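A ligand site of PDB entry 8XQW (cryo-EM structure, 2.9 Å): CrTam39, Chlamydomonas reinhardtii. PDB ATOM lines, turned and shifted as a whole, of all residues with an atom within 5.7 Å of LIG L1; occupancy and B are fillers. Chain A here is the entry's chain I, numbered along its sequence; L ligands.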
ATOM      1  N   PHE A 223     -13.296  22.064  31.131  1.00  0.00           N
ATOM      2  CA  PHE A 223     -12.680  22.734  29.996  1.00  0.00           C
ATOM      3  C   PHE A 223     -13.020  22.034  28.683  1.00  0.00           C
ATOM      4  O   PHE A 223     -13.204  22.692  27.658  1.00  0.00           O
ATOM      5  CB  PHE A 223     -11.173  22.820  30.158  1.00  0.00           C
ATOM      6  CG  PHE A 223     -10.512  23.714  29.159  1.00  0.00           C
ATOM      7  CD1 PHE A 223     -10.954  25.004  28.988  1.00  0.00           C
ATOM      8  CD2 PHE A 223      -9.472  23.253  28.391  1.00  0.00           C
ATOM      9  CE1 PHE A 223     -10.362  25.824  28.057  1.00  0.00           C
ATOM     10  CE2 PHE A 223      -8.882  24.076  27.473  1.00  0.00           C
ATOM     11  CZ  PHE A 223      -9.331  25.357  27.309  1.00  0.00           C
ATOM     12  N   ILE A 226     -16.507  23.204  27.776  1.00  0.00           N
ATOM     13  CA  ILE A 226     -16.473  24.592  27.314  1.00  0.00           C
ATOM     14  C   ILE A 226     -15.928  24.665  25.899  1.00  0.00           C
ATOM     15  O   ILE A 226     -16.510  25.331  25.043  1.00  0.00           O
ATOM     16  CB  ILE A 226     -15.631  25.435  28.275  1.00  0.00           C
ATOM     17  CG1 ILE A 226     -16.353  25.637  29.587  1.00  0.00           C
ATOM     18  CG2 ILE A 226     -15.351  26.761  27.659  1.00  0.00           C
ATOM     19  CD1 ILE A 226     -15.512  26.319  30.618  1.00  0.00           C
ATOM     20  N   MET A 227     -14.805  23.997  25.628  1.00  0.00           N
ATOM     21  CA  MET A 227     -14.248  24.013  24.283  1.00  0.00           C
ATOM     22  C   MET A 227     -15.254  23.502  23.262  1.00  0.00           C
ATOM     23  O   MET A 227     -15.457  24.131  22.225  1.00  0.00           O
ATOM     24  CB  MET A 227     -12.981  23.167  24.217  1.00  0.00           C
ATOM     25  CG  MET A 227     -11.799  23.748  24.941  1.00  0.00           C
ATOM     26  SD  MET A 227     -10.912  24.985  23.999  1.00  0.00           S
ATOM     27  CE  MET A 227     -10.538  24.077  22.513  1.00  0.00           C
ATOM     28  N   ALA A 228     -15.886  22.363  23.538  1.00  0.00           N
ATOM     29  CA  ALA A 228     -16.808  21.790  22.556  1.00  0.00           C
ATOM     30  C   ALA A 228     -17.999  22.708  22.302  1.00  0.00           C
ATOM     31  O   ALA A 228     -18.343  22.990  21.149  1.00  0.00           O
ATOM     32  CB  ALA A 228     -17.290  20.419  23.025  1.00  0.00           C
ATOM     33  N   ALA A 229     -18.633  23.191  23.370  1.00  0.00           N
ATOM     34  CA  ALA A 229     -19.784  24.063  23.210  1.00  0.00           C
ATOM     35  C   ALA A 229     -19.421  25.331  22.457  1.00  0.00           C
ATOM     36  O   ALA A 229     -20.114  25.718  21.507  1.00  0.00           O
ATOM     37  CB  ALA A 229     -20.378  24.427  24.565  1.00  0.00           C
ATOM     38  N   GLY A 230     -18.337  25.995  22.861  1.00  0.00           N
ATOM     39  CA  GLY A 230     -17.941  27.229  22.199  1.00  0.00           C
ATOM     40  C   GLY A 230     -17.576  27.021  20.753  1.00  0.00           C
ATOM     41  O   GLY A 230     -17.919  27.835  19.894  1.00  0.00           O
ATOM     42  N   GLY A 231     -16.886  25.927  20.436  1.00  0.00           N
ATOM     43  CA  GLY A 231     -16.524  25.669  19.056  1.00  0.00           C
ATOM     44  C   GLY A 231     -17.738  25.479  18.181  1.00  0.00           C
ATOM     45  O   GLY A 231     -17.835  26.061  17.102  1.00  0.00           O
ATOM     46  N   THR A 234     -19.712  28.858  17.824  1.00  0.00           N
ATOM     47  CA  THR A 234     -19.037  29.796  16.944  1.00  0.00           C
ATOM     48  C   THR A 234     -19.140  29.357  15.493  1.00  0.00           C
ATOM     49  O   THR A 234     -19.477  30.162  14.615  1.00  0.00           O
ATOM     50  CB  THR A 234     -17.583  29.952  17.361  1.00  0.00           C
ATOM     51  OG1 THR A 234     -17.491  30.884  18.444  1.00  0.00           O
ATOM     52  CG2 THR A 234     -16.748  30.458  16.208  1.00  0.00           C
ATOM     53  N   GLU A 242     -13.222  25.830  10.974  1.00  0.00           N
ATOM     54  CA  GLU A 242     -12.115  25.500  11.848  1.00  0.00           C
ATOM     55  C   GLU A 242     -12.504  25.556  13.316  1.00  0.00           C
ATOM     56  O   GLU A 242     -12.055  24.700  14.089  1.00  0.00           O
ATOM     57  CB  GLU A 242     -10.927  26.428  11.578  1.00  0.00           C
ATOM     58  CG  GLU A 242      -9.752  26.204  12.488  1.00  0.00           C
ATOM     59  CD  GLU A 242      -8.943  27.456  12.714  1.00  0.00           C
ATOM     60  OE1 GLU A 242      -7.795  27.517  12.244  1.00  0.00           O
ATOM     61  OE2 GLU A 242      -9.449  28.383  13.364  1.00  0.00           O
ATOM     62  N   PRO A 243     -13.302  26.533  13.766  1.00  0.00           N
ATOM     63  CA  PRO A 243     -13.673  26.538  15.188  1.00  0.00           C
ATOM     64  C   PRO A 243     -14.285  25.244  15.674  1.00  0.00           C
ATOM     65  O   PRO A 243     -13.853  24.737  16.720  1.00  0.00           O
ATOM     66  CB  PRO A 243     -14.657  27.709  15.286  1.00  0.00           C
ATOM     67  CG  PRO A 243     -14.899  28.150  13.919  1.00  0.00           C
ATOM     68  CD  PRO A 243     -13.695  27.791  13.137  1.00  0.00           C
ATOM     69  N   VAL A 244     -15.264  24.679  14.972  1.00  0.00           N
ATOM     70  CA  VAL A 244     -15.904  23.461  15.463  1.00  0.00           C
ATOM     71  C   VAL A 244     -14.945  22.288  15.404  1.00  0.00           C
ATOM     72  O   VAL A 244     -14.946  21.440  16.288  1.00  0.00           O
ATOM     73  CB  VAL A 244     -17.212  23.173  14.706  1.00  0.00           C
ATOM     74  CG1 VAL A 244     -16.940  22.652  13.320  1.00  0.00           C
ATOM     75  CG2 VAL A 244     -18.034  22.186  15.485  1.00  0.00           C
ATOM     76  N   ALA A 246     -11.545  22.247  15.628  1.00  0.00           N
ATOM     77  CA  ALA A 246     -10.600  22.337  16.732  1.00  0.00           C
ATOM     78  C   ALA A 246     -11.282  22.127  18.062  1.00  0.00           C
ATOM     79  O   ALA A 246     -10.772  21.403  18.924  1.00  0.00           O
ATOM     80  CB  ALA A 246      -9.887  23.680  16.703  1.00  0.00           C
ATOM     81  N   GLY A 247     -12.455  22.727  18.257  1.00  0.00           N
ATOM     82  CA  GLY A 247     -13.145  22.605  19.534  1.00  0.00           C
ATOM     83  C   GLY A 247     -13.571  21.190  19.845  1.00  0.00           C
ATOM     84  O   GLY A 247     -13.383  20.710  20.964  1.00  0.00           O
ATOM     85  N   GLU A 287      -2.923  29.472  19.687  1.00  0.00           N
ATOM     86  CA  GLU A 287      -3.483  30.780  19.959  1.00  0.00           C
ATOM     87  C   GLU A 287      -2.439  31.877  19.871  1.00  0.00           C
ATOM     88  O   GLU A 287      -2.672  32.891  19.213  1.00  0.00           O
ATOM     89  CB  GLU A 287      -4.142  30.806  21.318  1.00  0.00           C
ATOM     90  CG  GLU A 287      -4.421  32.196  21.787  1.00  0.00           C
ATOM     91  CD  GLU A 287      -5.789  32.334  22.356  1.00  0.00           C
ATOM     92  OE1 GLU A 287      -6.715  31.685  21.828  1.00  0.00           O
ATOM     93  OE2 GLU A 287      -5.961  33.092  23.325  1.00  0.00           O
ATOM     94  N   TRP A 292      -6.452  32.469  15.235  1.00  0.00           N
ATOM     95  CA  TRP A 292      -7.644  31.783  14.760  1.00  0.00           C
ATOM     96  C   TRP A 292      -8.124  32.378  13.445  1.00  0.00           C
ATOM     97  O   TRP A 292      -8.003  33.585  13.224  1.00  0.00           O
ATOM     98  CB  TRP A 292      -8.754  31.857  15.801  1.00  0.00           C
ATOM     99  CG  TRP A 292      -8.353  31.352  17.117  1.00  0.00           C
ATOM    100  CD1 TRP A 292      -7.944  32.081  18.182  1.00  0.00           C
ATOM    101  CD2 TRP A 292      -8.308  29.991  17.528  1.00  0.00           C
ATOM    102  NE1 TRP A 292      -7.654  31.256  19.237  1.00  0.00           N
ATOM    103  CE2 TRP A 292      -7.872  29.968  18.862  1.00  0.00           C
ATOM    104  CE3 TRP A 292      -8.614  28.777  16.909  1.00  0.00           C
ATOM    105  CZ2 TRP A 292      -7.717  28.791  19.572  1.00  0.00           C
ATOM    106  CZ3 TRP A 292      -8.458  27.622  17.608  1.00  0.00           C
ATOM    107  CH2 TRP A 292      -8.014  27.630  18.924  1.00  0.00           C
ATOM    108  N   HIS A 294     -11.189  32.784  12.196  1.00  0.00           N
ATOM    109  CA  HIS A 294     -12.336  33.665  12.231  1.00  0.00           C
ATOM    110  C   HIS A 294     -12.045  34.991  12.908  1.00  0.00           C
ATOM    111  O   HIS A 294     -12.980  35.727  13.211  1.00  0.00           O
ATOM    112  CB  HIS A 294     -13.495  32.973  12.944  1.00  0.00           C
ATOM    113  CG  HIS A 294     -13.336  32.900  14.432  1.00  0.00           C
ATOM    114  ND1 HIS A 294     -12.412  32.082  15.034  1.00  0.00           N
ATOM    115  CD2 HIS A 294     -13.978  33.539  15.429  1.00  0.00           C
ATOM    116  CE1 HIS A 294     -12.494  32.219  16.347  1.00  0.00           C
ATOM    117  NE2 HIS A 294     -13.434  33.104  16.610  1.00  0.00           N
ATOM    118  N   LYS A 295     -10.777  35.313  13.160  1.00  0.00           N
ATOM    119  CA  LYS A 295     -10.411  36.534  13.852  1.00  0.00           C
ATOM    120  C   LYS A 295      -9.535  37.428  12.981  1.00  0.00           C
ATOM    121  O   LYS A 295      -8.826  38.286  13.483  1.00  0.00           O
ATOM    122  CB  LYS A 295      -9.719  36.230  15.172  1.00  0.00           C
ATOM    123  CG  LYS A 295     -10.681  35.829  16.251  1.00  0.00           C
ATOM    124  CD  LYS A 295     -10.227  36.300  17.591  1.00  0.00           C
ATOM    125  CE  LYS A 295     -11.422  36.610  18.449  1.00  0.00           C
ATOM    126  NZ  LYS A 295     -11.038  37.132  19.777  1.00  0.00           N
ATOM    127  N   GLU A 308      -5.599  35.513  24.344  1.00  0.00           N
ATOM    128  CA  GLU A 308      -6.929  36.017  24.755  1.00  0.00           C
ATOM    129  C   GLU A 308      -7.416  35.219  25.961  1.00  0.00           C
ATOM    130  O   GLU A 308      -6.673  35.167  26.956  1.00  0.00           O
ATOM    131  CB  GLU A 308      -7.860  35.889  23.565  1.00  0.00           C
ATOM    132  CG  GLU A 308      -7.189  36.274  22.248  1.00  0.00           C
ATOM    133  CD  GLU A 308      -7.892  35.747  21.016  1.00  0.00           C
ATOM    134  OE1 GLU A 308      -7.731  34.546  20.700  1.00  0.00           O
ATOM    135  OE2 GLU A 308      -8.601  36.543  20.386  1.00  0.00           O
ATOM    136  N   LEU A 309      -8.594  34.605  25.881  1.00  0.00           N
ATOM    137  CA  LEU A 309      -9.146  33.935  27.084  1.00  0.00           C
ATOM    138  C   LEU A 309      -9.014  32.407  26.971  1.00  0.00           C
ATOM    139  O   LEU A 309      -8.829  31.769  28.008  1.00  0.00           O
ATOM    140  CB  LEU A 309     -10.589  34.381  27.285  1.00  0.00           C
ATOM    141  CG  LEU A 309     -10.849  35.229  28.530  1.00  0.00           C
ATOM    142  CD1 LEU A 309     -12.261  34.997  29.032  1.00  0.00           C
ATOM    143  CD2 LEU A 309      -9.834  34.877  29.604  1.00  0.00           C
ATOM    144  N   THR A 310      -9.097  31.853  25.768  1.00  0.00           N
ATOM    145  CA  THR A 310      -8.887  30.423  25.600  1.00  0.00           C
ATOM    146  C   THR A 310      -7.450  30.034  25.875  1.00  0.00           C
ATOM    147  O   THR A 310      -7.173  29.078  26.617  1.00  0.00           O
ATOM    148  CB  THR A 310      -9.304  29.997  24.207  1.00  0.00           C
ATOM    149  OG1 THR A 310     -10.725  29.835  24.158  1.00  0.00           O
ATOM    150  CG2 THR A 310      -8.667  28.684  23.831  1.00  0.00           C
ATOM    151  N   GLY A 311      -6.505  30.755  25.276  1.00  0.00           N
ATOM    152  CA  GLY A 311      -5.106  30.506  25.572  1.00  0.00           C
ATOM    153  C   GLY A 311      -4.782  30.663  27.040  1.00  0.00           C
ATOM    154  O   GLY A 311      -3.961  29.925  27.582  1.00  0.00           O
ATOM    155  N   ALA A 313      -6.825  30.146  29.646  1.00  0.00           N
ATOM    156  CA  ALA A 313      -7.337  28.995  30.385  1.00  0.00           C
ATOM    157  C   ALA A 313      -6.457  27.782  30.154  1.00  0.00           C
ATOM    158  O   ALA A 313      -6.162  27.029  31.097  1.00  0.00           O
ATOM    159  CB  ALA A 313      -8.773  28.691  29.981  1.00  0.00           C
HETATM  160  C1  LIG L   1     -17.158  29.963  25.065  1.00  0.00           C
HETATM  161  C2  LIG L   1     -18.443  29.221  25.042  1.00  0.00           C
HETATM  162  C3  LIG L   1     -18.947  29.004  26.444  1.00  0.00           C
HETATM  163  C4  LIG L   1     -19.998  27.911  26.429  1.00  0.00           C
HETATM  164  O1  LIG L   1     -16.748  30.746  25.889  1.00  0.00           O
HETATM  165  C5  LIG L   1     -13.692  30.799  26.167  1.00  0.00           C
HETATM  166  C6  LIG L   1     -12.973  30.408  27.405  1.00  0.00           C
HETATM  167  C7  LIG L   1     -13.809  30.695  28.604  1.00  0.00           C
HETATM  168  C8  LIG L   1     -13.004  31.473  29.606  1.00  0.00           C
HETATM  169  C9  LIG L   1     -12.528  30.427  30.568  1.00  0.00           C
HETATM  170  C10 LIG L   1     -13.275  30.678  31.868  1.00  0.00           C
HETATM  171  O2  LIG L   1     -13.562  31.860  25.594  1.00  0.00           O
HETATM  172  O3  LIG L   1     -16.312  29.368  24.202  1.00  0.00           O
HETATM  173  C11 LIG L   1     -15.391  30.144  23.547  1.00  0.00           C
HETATM  174  C12 LIG L   1     -14.041  29.731  24.124  1.00  0.00           C
HETATM  175  O4  LIG L   1     -14.146  29.727  25.501  1.00  0.00           O
HETATM  176  C13 LIG L   1     -13.812  28.298  23.713  1.00  0.00           C
HETATM  177  O5  LIG L   1     -14.101  28.389  22.361  1.00  0.00           O
HETATM  178  C14 LIG L   1     -13.011  28.162  21.590  1.00  0.00           C
HETATM  179  C15 LIG L   1     -13.480  27.241  20.519  1.00  0.00           C
HETATM  180  O6  LIG L   1     -13.683  26.049  21.161  1.00  0.00           O
HETATM  181  C16 LIG L   1     -12.273  27.068  19.633  1.00  0.00           C
HETATM  182  O7  LIG L   1     -12.658  26.314  18.547  1.00  0.00           O
HETATM  183  C17 LIG L   1     -11.887  28.442  19.069  1.00  0.00           C
HETATM  184  O8  LIG L   1     -12.942  28.974  18.387  1.00  0.00           O
HETATM  185  C18 LIG L   1     -11.688  29.415  20.234  1.00  0.00           C
HETATM  186  O9  LIG L   1     -11.571  31.613  20.903  1.00  0.00           O
HETATM  187  C19 LIG L   1     -11.632  30.832  19.749  1.00  0.00           C
HETATM  188  O10 LIG L   1     -12.807  29.407  21.026  1.00  0.00           O
HETATM  189  C20 LIG L   1     -11.348  32.955  20.667  1.00  0.00           C
HETATM  190  C21 LIG L   1     -10.904  33.648  21.976  1.00  0.00           C
HETATM  191  O11 LIG L   1      -9.942  32.832  22.510  1.00  0.00           O
HETATM  192  C22 LIG L   1     -12.056  33.748  22.948  1.00  0.00           C
HETATM  193  O12 LIG L   1     -11.594  34.605  23.934  1.00  0.00           O
HETATM  194  C23 LIG L   1     -13.224  34.416  22.254  1.00  0.00           C
HETATM  195  O13 LIG L   1     -12.799  35.602  21.699  1.00  0.00           O
HETATM  196  C24 LIG L   1     -13.602  33.527  21.098  1.00  0.00           C
HETATM  197  O14 LIG L   1     -12.558  33.454  20.192  1.00  0.00           O
HETATM  198  C25 LIG L   1     -14.722  34.122  20.242  1.00  0.00           C
HETATM  199  O15 LIG L   1     -14.585  33.514  19.003  1.00  0.00           O
HETATM  200  C1  LG2 L   2      -2.337  18.893  46.063  1.00  0.00           C
HETATM  201  O1  LG2 L   2      -3.557  19.574  46.019  1.00  0.00           O
HETATM  202  C2  LG2 L   2      -1.992  18.912  47.586  1.00  0.00           C
HETATM  203  O2  LG2 L   2      -1.280  20.095  47.758  1.00  0.00           O
HETATM  204  C3  LG2 L   2      -1.020  17.771  47.923  1.00  0.00           C
HETATM  205  O3  LG2 L   2      -1.054  17.691  49.310  1.00  0.00           O
HETATM  206  C4  LG2 L   2      -1.537  16.460  47.332  1.00  0.00           C
HETATM  207  O4  LG2 L   2      -2.808  16.213  47.850  1.00  0.00           O
HETATM  208  C5  LG2 L   2      -1.696  16.691  45.831  1.00  0.00           C
HETATM  209  O5  LG2 L   2      -2.000  15.530  43.818  1.00  0.00           O
HETATM  210  C6  LG2 L   2      -2.112  15.362  45.193  1.00  0.00           C
HETATM  211  O6  LG2 L   2      -2.699  17.611  45.607  1.00  0.00           O
HETATM  212  C7  LG2 L   2      -3.716  20.392  44.905  1.00  0.00           C
HETATM  213  C8  LG2 L   2      -4.723  21.450  45.346  1.00  0.00           C
HETATM  214  C9  LG2 L   2      -3.961  22.579  46.021  1.00  0.00           C
HETATM  215  O7  LG2 L   2      -5.295  22.005  44.184  1.00  0.00           O
HETATM  216  C10 LG2 L   2      -6.509  21.549  43.803  1.00  0.00           C
HETATM  217  O8  LG2 L   2      -7.069  20.740  44.521  1.00  0.00           O
HETATM  218  C11 LG2 L   2      -6.776  21.764  42.354  1.00  0.00           C
HETATM  219  C12 LG2 L   2      -6.795  23.223  41.995  1.00  0.00           C
HETATM  220  C13 LG2 L   2      -7.100  23.425  40.535  1.00  0.00           C
HETATM  221  C14 LG2 L   2      -6.780  24.857  40.176  1.00  0.00           C
HETATM  222  C15 LG2 L   2      -6.554  24.925  38.690  1.00  0.00           C
HETATM  223  C16 LG2 L   2      -7.128  26.215  38.158  1.00  0.00           C
HETATM  224  C17 LG2 L   2      -6.937  26.220  36.678  1.00  0.00           C
HETATM  225  C18 LG2 L   2      -8.272  25.900  36.074  1.00  0.00           C
HETATM  226  C19 LG2 L   2      -8.551  26.904  35.005  1.00  0.00           C
HETATM  227  C20 LG2 L   2      -9.243  26.139  33.902  1.00  0.00           C
HETATM  228  C21 LG2 L   2     -10.575  26.775  33.703  1.00  0.00           C
HETATM  229  C22 LG2 L   2     -11.347  25.791  32.915  1.00  0.00           C
HETATM  230  C23 LG2 L   2     -12.765  25.915  33.334  1.00  0.00           C
HETATM  231  O9  LG2 L   2      -3.958  23.648  45.115  1.00  0.00           O
HETATM  232  C24 LG2 L   2      -2.844  23.833  44.394  1.00  0.00           C
HETATM  233  O10 LG2 L   2      -1.896  23.076  44.539  1.00  0.00           O
HETATM  234  C25 LG2 L   2      -2.808  25.122  43.659  1.00  0.00           C
HETATM  235  C26 LG2 L   2      -2.150  24.943  42.304  1.00  0.00           C
HETATM  236  C27 LG2 L   2      -2.472  26.171  41.509  1.00  0.00           C
HETATM  237  C28 LG2 L   2      -2.211  25.833  40.069  1.00  0.00           C
HETATM  238  C29 LG2 L   2      -3.336  26.408  39.274  1.00  0.00           C
HETATM  239  C30 LG2 L   2      -2.791  27.511  38.403  1.00  0.00           C
HETATM  240  C31 LG2 L   2      -3.618  28.740  38.727  1.00  0.00           C
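O7 of LIG L1 is in hydrogen-bond range of O of Pro 243 (2.7 Å).
NE2 of His 294 lies within hydrogen-bond range of O15 of LIG L1, at 2.7 Å.
OE1 of Glu 287 sits at hydrogen-bond distance from O11 of LIG L1 (3.5 Å).
The backbone NH (N) of Gly 231 sits at hydrogen-bond distance from an oxygen (O6) of LIG L1.
An oxygen (O11) of LIG L1 sits at hydrogen-bond distance from the side-chain carboxylate (OE1) of Glu 308 (3.3 Å).
O of Met 227 is in hydrogen-bond range of O6 of LIG L1 (2.8 Å).
NZ of Lys 295 is in hydrogen-bond range of O13 of LIG L1, at 3.0 Å.
The indole nitrogen (NE1) of Trp 292 is in hydrogen-bond range of the side-chain carboxylate (OE1) of Glu 287 (2.8 Å).
The side-chain carboxylate of Glu 287 sits at hydrogen-bond distance from the backbone NH of Gly 311, 3.1 Å away.
N of Glu 308 is in hydrogen-bond range of OE2 of Glu 287 (2.7 Å).
OG1 of Thr 234 lies close to O of Gly 230 (3.4 Å).
The side-chain amino group (NZ) of Lys 295 lies within salt-bridge range of the side-chain carboxylate (OE2) of Glu 308 (2.6 Å).
Merely in contact with LIG L1: Thr 310, Gly 230, Leu 309, Gly 247, Trp 292, Ile 226, Thr 234 and Ala 229.
Hydrophobic or aromatic side chains that line LIG L1: Ile 226, Met 227, Ala 229, Pro 243, Trp 292, His 294 and Leu 309.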
